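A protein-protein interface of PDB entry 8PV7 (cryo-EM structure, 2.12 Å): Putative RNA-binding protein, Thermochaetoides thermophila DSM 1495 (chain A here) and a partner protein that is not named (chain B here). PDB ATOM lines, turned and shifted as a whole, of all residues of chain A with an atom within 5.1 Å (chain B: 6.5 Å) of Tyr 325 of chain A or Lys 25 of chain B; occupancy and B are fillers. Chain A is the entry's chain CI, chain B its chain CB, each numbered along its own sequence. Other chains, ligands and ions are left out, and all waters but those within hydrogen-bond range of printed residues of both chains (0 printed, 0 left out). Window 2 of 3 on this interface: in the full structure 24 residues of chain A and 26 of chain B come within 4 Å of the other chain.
NZ of Lys 321 of chain A lies within salt-bridge range of OE1 of Glu 326 of chain A, 2.8 Å away.
Of the 15 printed residues of chain B, 7 touch a printed residue of chain A.
Printed residues of chain B that touch a printed residue of chain A: Gln 22, Lys 25, Ala 26, Ala 290, Leu 291, Pro 292 and Ile 293.
Hydrophobic or aromatic side chains of chain A that line the printed part of chain B: Leu 320, Met 323, Tyr 325 and Phe 327.
Among the printed residues, no Asp or Glu carboxylate lies within 4 Å of a Lys or Arg side-chain nitrogen of the other chain.
Of the printed residues of chain B, Leu 320 of chain A touches Ala 290, Leu 291 and Pro 292.
Printed residues of chain B within 4 Å of Met 323 of chain A: Leu 291.
Of the printed residues of chain B, Tyr 325 of chain A touches Gln 22, Lys 25, Ala 26 and Pro 292.
Printed residues of chain A within 4 Å of Lys 25 of chain B: Tyr 325 (3.99 Å).
Cys 27 of chain B touches none of the printed residues of chain A.
Leu 30 of chain B touches none of the printed residues of chain A.
Printed residues of chain A within 4 Å of Ala 290 of chain B: Leu 320 (3.6 Å).
Of the printed residues of chain A, Ile 293 of chain B touches Phe 327 (3.5 Å).
NE2 of Gln 22 of chain B lies close to OH of Tyr 325 of chain A, 3.5 Å away.
The side-chain amide nitrogen (NE2) of Gln 22 of chain B lies within hydrogen-bond range of the backbone carbonyl oxygen (O) of Glu 326 of chain A (2.8 Å).
OH of Tyr 325 of chain A sits at hydrogen-bond distance from O of Pro 292 of chain B.
CD2 of Leu 320 of chain A touches O of Ala 290 of chain B (3.6 Å).
Leu 320 of chain A touches Leu 291 of chain B.
Pro 292 of chain B touches Leu 320 of chain A (CD to CD1, 3.6 Å).
CE of Met 323 of chain A touches CD2 of Leu 291 of chain B (3.7 Å).
Lys 25 of chain B touches Tyr 325 of chain A (C to CE1, 3.99 Å).
Tyr 325 of chain A touches Ala 26 of chain B.
Gln 22 of chain B touches Phe 327 of chain A (CD to CD1, 3.5 Å).
CD1 of Phe 327 of chain A touches O of Pro 292 of chain B, 3.2 Å away.
CE1 of Phe 327 of chain A touches O of Ile 293 of chain B, 3.5 Å away.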
ATOM      1  N   LEU A 320     -14.886 -28.279  -0.760  1.00  0.00           N
ATOM      2  CA  LEU A 320     -14.048 -27.090  -0.637  1.00  0.00           C
ATOM      3  C   LEU A 320     -14.124 -26.211  -1.871  1.00  0.00           C
ATOM      4  O   LEU A 320     -13.814 -25.017  -1.800  1.00  0.00           O
ATOM      5  CB  LEU A 320     -12.590 -27.474  -0.403  1.00  0.00           C
ATOM      6  CG  LEU A 320     -12.147 -28.183   0.868  1.00  0.00           C
ATOM      7  CD1 LEU A 320     -10.660 -28.427   0.780  1.00  0.00           C
ATOM      8  CD2 LEU A 320     -12.515 -27.396   2.097  1.00  0.00           C
ATOM      9  N   LYS A 321     -14.489 -26.795  -3.016  1.00  0.00           N
ATOM     10  CA  LYS A 321     -14.515 -26.034  -4.265  1.00  0.00           C
ATOM     11  C   LYS A 321     -15.525 -24.888  -4.240  1.00  0.00           C
ATOM     12  O   LYS A 321     -15.363 -23.913  -4.982  1.00  0.00           O
ATOM     13  CB  LYS A 321     -14.803 -26.976  -5.436  1.00  0.00           C
ATOM     14  CG  LYS A 321     -14.362 -26.463  -6.810  1.00  0.00           C
ATOM     15  CD  LYS A 321     -12.990 -25.786  -6.830  1.00  0.00           C
ATOM     16  CE  LYS A 321     -11.843 -26.743  -6.510  1.00  0.00           C
ATOM     17  NZ  LYS A 321     -10.552 -26.012  -6.434  1.00  0.00           N
ATOM     18  N   MET A 323     -15.967 -22.920  -1.620  1.00  0.00           N
ATOM     19  CA  MET A 323     -15.385 -21.838  -0.836  1.00  0.00           C
ATOM     20  C   MET A 323     -14.216 -21.157  -1.533  1.00  0.00           C
ATOM     21  O   MET A 323     -13.687 -20.178  -0.998  1.00  0.00           O
ATOM     22  CB  MET A 323     -14.931 -22.357   0.529  1.00  0.00           C
ATOM     23  CG  MET A 323     -16.007 -23.110   1.297  1.00  0.00           C
ATOM     24  SD  MET A 323     -15.623 -23.426   3.034  1.00  0.00           S
ATOM     25  CE  MET A 323     -14.209 -22.361   3.304  1.00  0.00           C
ATOM     26  N   GLY A 324     -13.801 -21.642  -2.699  1.00  0.00           N
ATOM     27  CA  GLY A 324     -12.684 -21.046  -3.397  1.00  0.00           C
ATOM     28  C   GLY A 324     -11.326 -21.508  -2.930  1.00  0.00           C
ATOM     29  O   GLY A 324     -10.339 -20.790  -3.119  1.00  0.00           O
ATOM     30  N   TYR A 325     -11.241 -22.687  -2.322  1.00  0.00           N
ATOM     31  CA  TYR A 325      -9.984 -23.242  -1.844  1.00  0.00           C
ATOM     32  C   TYR A 325      -9.614 -24.482  -2.641  1.00  0.00           C
ATOM     33  O   TYR A 325     -10.462 -25.342  -2.896  1.00  0.00           O
ATOM     34  CB  TYR A 325     -10.056 -23.570  -0.353  1.00  0.00           C
ATOM     35  CG  TYR A 325      -8.727 -23.991   0.219  1.00  0.00           C
ATOM     36  CD1 TYR A 325      -7.694 -23.083   0.367  1.00  0.00           C
ATOM     37  CD2 TYR A 325      -8.518 -25.297   0.635  1.00  0.00           C
ATOM     38  CE1 TYR A 325      -6.478 -23.473   0.881  1.00  0.00           C
ATOM     39  CE2 TYR A 325      -7.307 -25.691   1.164  1.00  0.00           C
ATOM     40  CZ  TYR A 325      -6.293 -24.774   1.288  1.00  0.00           C
ATOM     41  OH  TYR A 325      -5.082 -25.157   1.811  1.00  0.00           O
ATOM     42  N   GLU A 326      -8.345 -24.565  -3.030  1.00  0.00           N
ATOM     43  CA  GLU A 326      -7.801 -25.712  -3.742  1.00  0.00           C
ATOM     44  C   GLU A 326      -6.584 -26.225  -2.992  1.00  0.00           C
ATOM     45  O   GLU A 326      -5.625 -25.478  -2.771  1.00  0.00           O
ATOM     46  CB  GLU A 326      -7.429 -25.346  -5.180  1.00  0.00           C
ATOM     47  CG  GLU A 326      -7.128 -26.500  -6.175  1.00  0.00           C
ATOM     48  CD  GLU A 326      -7.944 -27.792  -6.003  1.00  0.00           C
ATOM     49  OE1 GLU A 326      -8.719 -28.104  -6.931  1.00  0.00           O
ATOM     50  OE2 GLU A 326      -7.748 -28.554  -5.028  1.00  0.00           O
ATOM     51  N   PHE A 327      -6.624 -27.496  -2.605  1.00  0.00           N
ATOM     52  CA  PHE A 327      -5.511 -28.161  -1.943  1.00  0.00           C
ATOM     53  C   PHE A 327      -5.100 -29.352  -2.790  1.00  0.00           C
ATOM     54  O   PHE A 327      -5.926 -30.222  -3.084  1.00  0.00           O
ATOM     55  CB  PHE A 327      -5.896 -28.602  -0.529  1.00  0.00           C
ATOM     56  CG  PHE A 327      -4.815 -29.359   0.187  1.00  0.00           C
ATOM     57  CD1 PHE A 327      -3.643 -28.728   0.567  1.00  0.00           C
ATOM     58  CD2 PHE A 327      -4.979 -30.698   0.494  1.00  0.00           C
ATOM     59  CE1 PHE A 327      -2.651 -29.421   1.229  1.00  0.00           C
ATOM     60  CE2 PHE A 327      -3.989 -31.397   1.155  1.00  0.00           C
ATOM     61  CZ  PHE A 327      -2.825 -30.758   1.523  1.00  0.00           C
ATOM     62  N   PRO B  20       4.088 -23.156   3.640  1.00  0.00           N
ATOM     63  CA  PRO B  20       3.561 -21.896   4.188  1.00  0.00           C
ATOM     64  C   PRO B  20       2.715 -21.099   3.211  1.00  0.00           C
ATOM     65  O   PRO B  20       1.814 -20.374   3.656  1.00  0.00           O
ATOM     66  CB  PRO B  20       4.828 -21.127   4.579  1.00  0.00           C
ATOM     67  CG  PRO B  20       5.877 -21.651   3.673  1.00  0.00           C
ATOM     68  CD  PRO B  20       5.539 -23.092   3.397  1.00  0.00           C
ATOM     69  N   ASP B  21       2.968 -21.208   1.906  1.00  0.00           N
ATOM     70  CA  ASP B  21       2.126 -20.526   0.927  1.00  0.00           C
ATOM     71  C   ASP B  21       0.712 -21.092   0.932  1.00  0.00           C
ATOM     72  O   ASP B  21      -0.269 -20.343   0.866  1.00  0.00           O
ATOM     73  CB  ASP B  21       2.748 -20.636  -0.464  1.00  0.00           C
ATOM     74  CG  ASP B  21       4.224 -20.294  -0.468  1.00  0.00           C
ATOM     75  OD1 ASP B  21       4.727 -19.820   0.572  1.00  0.00           O
ATOM     76  OD2 ASP B  21       4.880 -20.499  -1.511  1.00  0.00           O
ATOM     77  N   GLN B  22       0.591 -22.418   1.029  1.00  0.00           N
ATOM     78  CA  GLN B  22      -0.725 -23.039   1.119  1.00  0.00           C
ATOM     79  C   GLN B  22      -1.414 -22.687   2.431  1.00  0.00           C
ATOM     80  O   GLN B  22      -2.639 -22.527   2.465  1.00  0.00           O
ATOM     81  CB  GLN B  22      -0.595 -24.554   0.966  1.00  0.00           C
ATOM     82  CG  GLN B  22      -1.914 -25.280   0.825  1.00  0.00           C
ATOM     83  CD  GLN B  22      -2.141 -25.787  -0.582  1.00  0.00           C
ATOM     84  OE1 GLN B  22      -1.279 -26.447  -1.160  1.00  0.00           O
ATOM     85  NE2 GLN B  22      -3.302 -25.478  -1.145  1.00  0.00           N
ATOM     86  N   THR B  23      -0.641 -22.546   3.510  1.00  0.00           N
ATOM     87  CA  THR B  23      -1.193 -22.096   4.785  1.00  0.00           C
ATOM     88  C   THR B  23      -1.755 -20.683   4.670  1.00  0.00           C
ATOM     89  O   THR B  23      -2.844 -20.389   5.179  1.00  0.00           O
ATOM     90  CB  THR B  23      -0.112 -22.158   5.865  1.00  0.00           C
ATOM     91  OG1 THR B  23       0.403 -23.492   5.954  1.00  0.00           O
ATOM     92  CG2 THR B  23      -0.672 -21.749   7.214  1.00  0.00           C
ATOM     93  N   LEU B  24      -1.021 -19.797   3.993  1.00  0.00           N
ATOM     94  CA  LEU B  24      -1.493 -18.430   3.786  1.00  0.00           C
ATOM     95  C   LEU B  24      -2.744 -18.398   2.914  1.00  0.00           C
ATOM     96  O   LEU B  24      -3.673 -17.620   3.174  1.00  0.00           O
ATOM     97  CB  LEU B  24      -0.383 -17.588   3.162  1.00  0.00           C
ATOM     98  CG  LEU B  24      -0.666 -16.097   3.000  1.00  0.00           C
ATOM     99  CD1 LEU B  24      -1.113 -15.500   4.319  1.00  0.00           C
ATOM    100  CD2 LEU B  24       0.566 -15.383   2.479  1.00  0.00           C
ATOM    101  N   LYS B  25      -2.783 -19.237   1.875  1.00  0.00           N
ATOM    102  CA  LYS B  25      -3.973 -19.339   1.034  1.00  0.00           C
ATOM    103  C   LYS B  25      -5.171 -19.825   1.838  1.00  0.00           C
ATOM    104  O   LYS B  25      -6.291 -19.328   1.668  1.00  0.00           O
ATOM    105  CB  LYS B  25      -3.707 -20.275  -0.142  1.00  0.00           C
ATOM    106  CG  LYS B  25      -2.725 -19.738  -1.173  1.00  0.00           C
ATOM    107  CD  LYS B  25      -2.197 -20.817  -2.131  1.00  0.00           C
ATOM    108  CE  LYS B  25      -3.162 -21.979  -2.369  1.00  0.00           C
ATOM    109  NZ  LYS B  25      -4.425 -21.575  -3.060  1.00  0.00           N
ATOM    110  N   ALA B  26      -4.949 -20.801   2.722  1.00  0.00           N
ATOM    111  CA  ALA B  26      -6.022 -21.301   3.575  1.00  0.00           C
ATOM    112  C   ALA B  26      -6.513 -20.231   4.536  1.00  0.00           C
ATOM    113  O   ALA B  26      -7.720 -20.103   4.762  1.00  0.00           O
ATOM    114  CB  ALA B  26      -5.552 -22.534   4.341  1.00  0.00           C
ATOM    115  N   CYS B  27      -5.592 -19.455   5.110  1.00  0.00           N
ATOM    116  CA  CYS B  27      -5.985 -18.380   6.017  1.00  0.00           C
ATOM    117  C   CYS B  27      -6.819 -17.329   5.295  1.00  0.00           C
ATOM    118  O   CYS B  27      -7.856 -16.886   5.805  1.00  0.00           O
ATOM    119  CB  CYS B  27      -4.746 -17.750   6.648  1.00  0.00           C
ATOM    120  SG  CYS B  27      -3.881 -18.820   7.814  1.00  0.00           S
ATOM    121  N   LYS B  28      -6.396 -16.946   4.085  1.00  0.00           N
ATOM    122  CA  LYS B  28      -7.144 -15.959   3.309  1.00  0.00           C
ATOM    123  C   LYS B  28      -8.526 -16.475   2.920  1.00  0.00           C
ATOM    124  O   LYS B  28      -9.526 -15.761   3.067  1.00  0.00           O
ATOM    125  CB  LYS B  28      -6.352 -15.564   2.064  1.00  0.00           C
ATOM    126  CG  LYS B  28      -5.093 -14.774   2.362  1.00  0.00           C
ATOM    127  CD  LYS B  28      -4.668 -13.926   1.179  1.00  0.00           C
ATOM    128  CE  LYS B  28      -3.405 -14.472   0.535  1.00  0.00           C
ATOM    129  NZ  LYS B  28      -3.519 -15.918   0.204  1.00  0.00           N
ATOM    130  N   ALA B  29      -8.603 -17.723   2.445  1.00  0.00           N
ATOM    131  CA  ALA B  29      -9.887 -18.283   2.033  1.00  0.00           C
ATOM    132  C   ALA B  29     -10.828 -18.456   3.218  1.00  0.00           C
ATOM    133  O   ALA B  29     -12.028 -18.173   3.110  1.00  0.00           O
ATOM    134  CB  ALA B  29      -9.672 -19.616   1.320  1.00  0.00           C
ATOM    135  N   LEU B  30     -10.303 -18.905   4.361  1.00  0.00           N
ATOM    136  CA  LEU B  30     -11.125 -19.085   5.551  1.00  0.00           C
ATOM    137  C   LEU B  30     -11.632 -17.753   6.083  1.00  0.00           C
ATOM    138  O   LEU B  30     -12.796 -17.645   6.477  1.00  0.00           O
ATOM    139  CB  LEU B  30     -10.336 -19.821   6.632  1.00  0.00           C
ATOM    140  CG  LEU B  30     -11.149 -20.199   7.871  1.00  0.00           C
ATOM    141  CD1 LEU B  30     -12.288 -21.120   7.489  1.00  0.00           C
ATOM    142  CD2 LEU B  30     -10.270 -20.841   8.917  1.00  0.00           C
ATOM    143  N   ALA B 290     -13.405 -27.575   7.264  1.00  0.00           N
ATOM    144  CA  ALA B 290     -11.984 -27.693   7.560  1.00  0.00           C
ATOM    145  C   ALA B 290     -11.169 -27.664   6.274  1.00  0.00           C
ATOM    146  O   ALA B 290     -11.413 -28.455   5.358  1.00  0.00           O
ATOM    147  CB  ALA B 290     -11.709 -28.982   8.332  1.00  0.00           C
ATOM    148  N   LEU B 291     -10.201 -26.750   6.210  1.00  0.00           N
ATOM    149  CA  LEU B 291      -9.319 -26.638   5.061  1.00  0.00           C
ATOM    150  C   LEU B 291      -8.041 -27.403   5.357  1.00  0.00           C
ATOM    151  O   LEU B 291      -7.336 -27.054   6.314  1.00  0.00           O
ATOM    152  CB  LEU B 291      -9.001 -25.176   4.763  1.00  0.00           C
ATOM    153  CG  LEU B 291     -10.135 -24.154   4.818  1.00  0.00           C
ATOM    154  CD1 LEU B 291      -9.602 -22.773   4.510  1.00  0.00           C
ATOM    155  CD2 LEU B 291     -11.233 -24.505   3.857  1.00  0.00           C
ATOM    156  N   PRO B 292      -7.710 -28.446   4.602  1.00  0.00           N
ATOM    157  CA  PRO B 292      -6.450 -29.156   4.844  1.00  0.00           C
ATOM    158  C   PRO B 292      -5.256 -28.337   4.384  1.00  0.00           C
ATOM    159  O   PRO B 292      -5.207 -27.861   3.248  1.00  0.00           O
ATOM    160  CB  PRO B 292      -6.606 -30.441   4.023  1.00  0.00           C
ATOM    161  CG  PRO B 292      -7.635 -30.119   3.001  1.00  0.00           C
ATOM    162  CD  PRO B 292      -8.574 -29.160   3.653  1.00  0.00           C
ATOM    163  N   ILE B 293      -4.288 -28.174   5.280  1.00  0.00           N
ATOM    164  CA  ILE B 293      -3.030 -27.523   4.959  1.00  0.00           C
ATOM    165  C   ILE B 293      -1.899 -28.533   4.815  1.00  0.00           C
ATOM    166  O   ILE B 293      -0.937 -28.288   4.085  1.00  0.00           O
ATOM    167  CB  ILE B 293      -2.673 -26.443   6.002  1.00  0.00           C
ATOM    168  CG1 ILE B 293      -2.684 -27.016   7.415  1.00  0.00           C
ATOM    169  CG2 ILE B 293      -3.638 -25.288   5.905  1.00  0.00           C
ATOM    170  CD1 ILE B 293      -2.243 -26.024   8.461  1.00  0.00           C
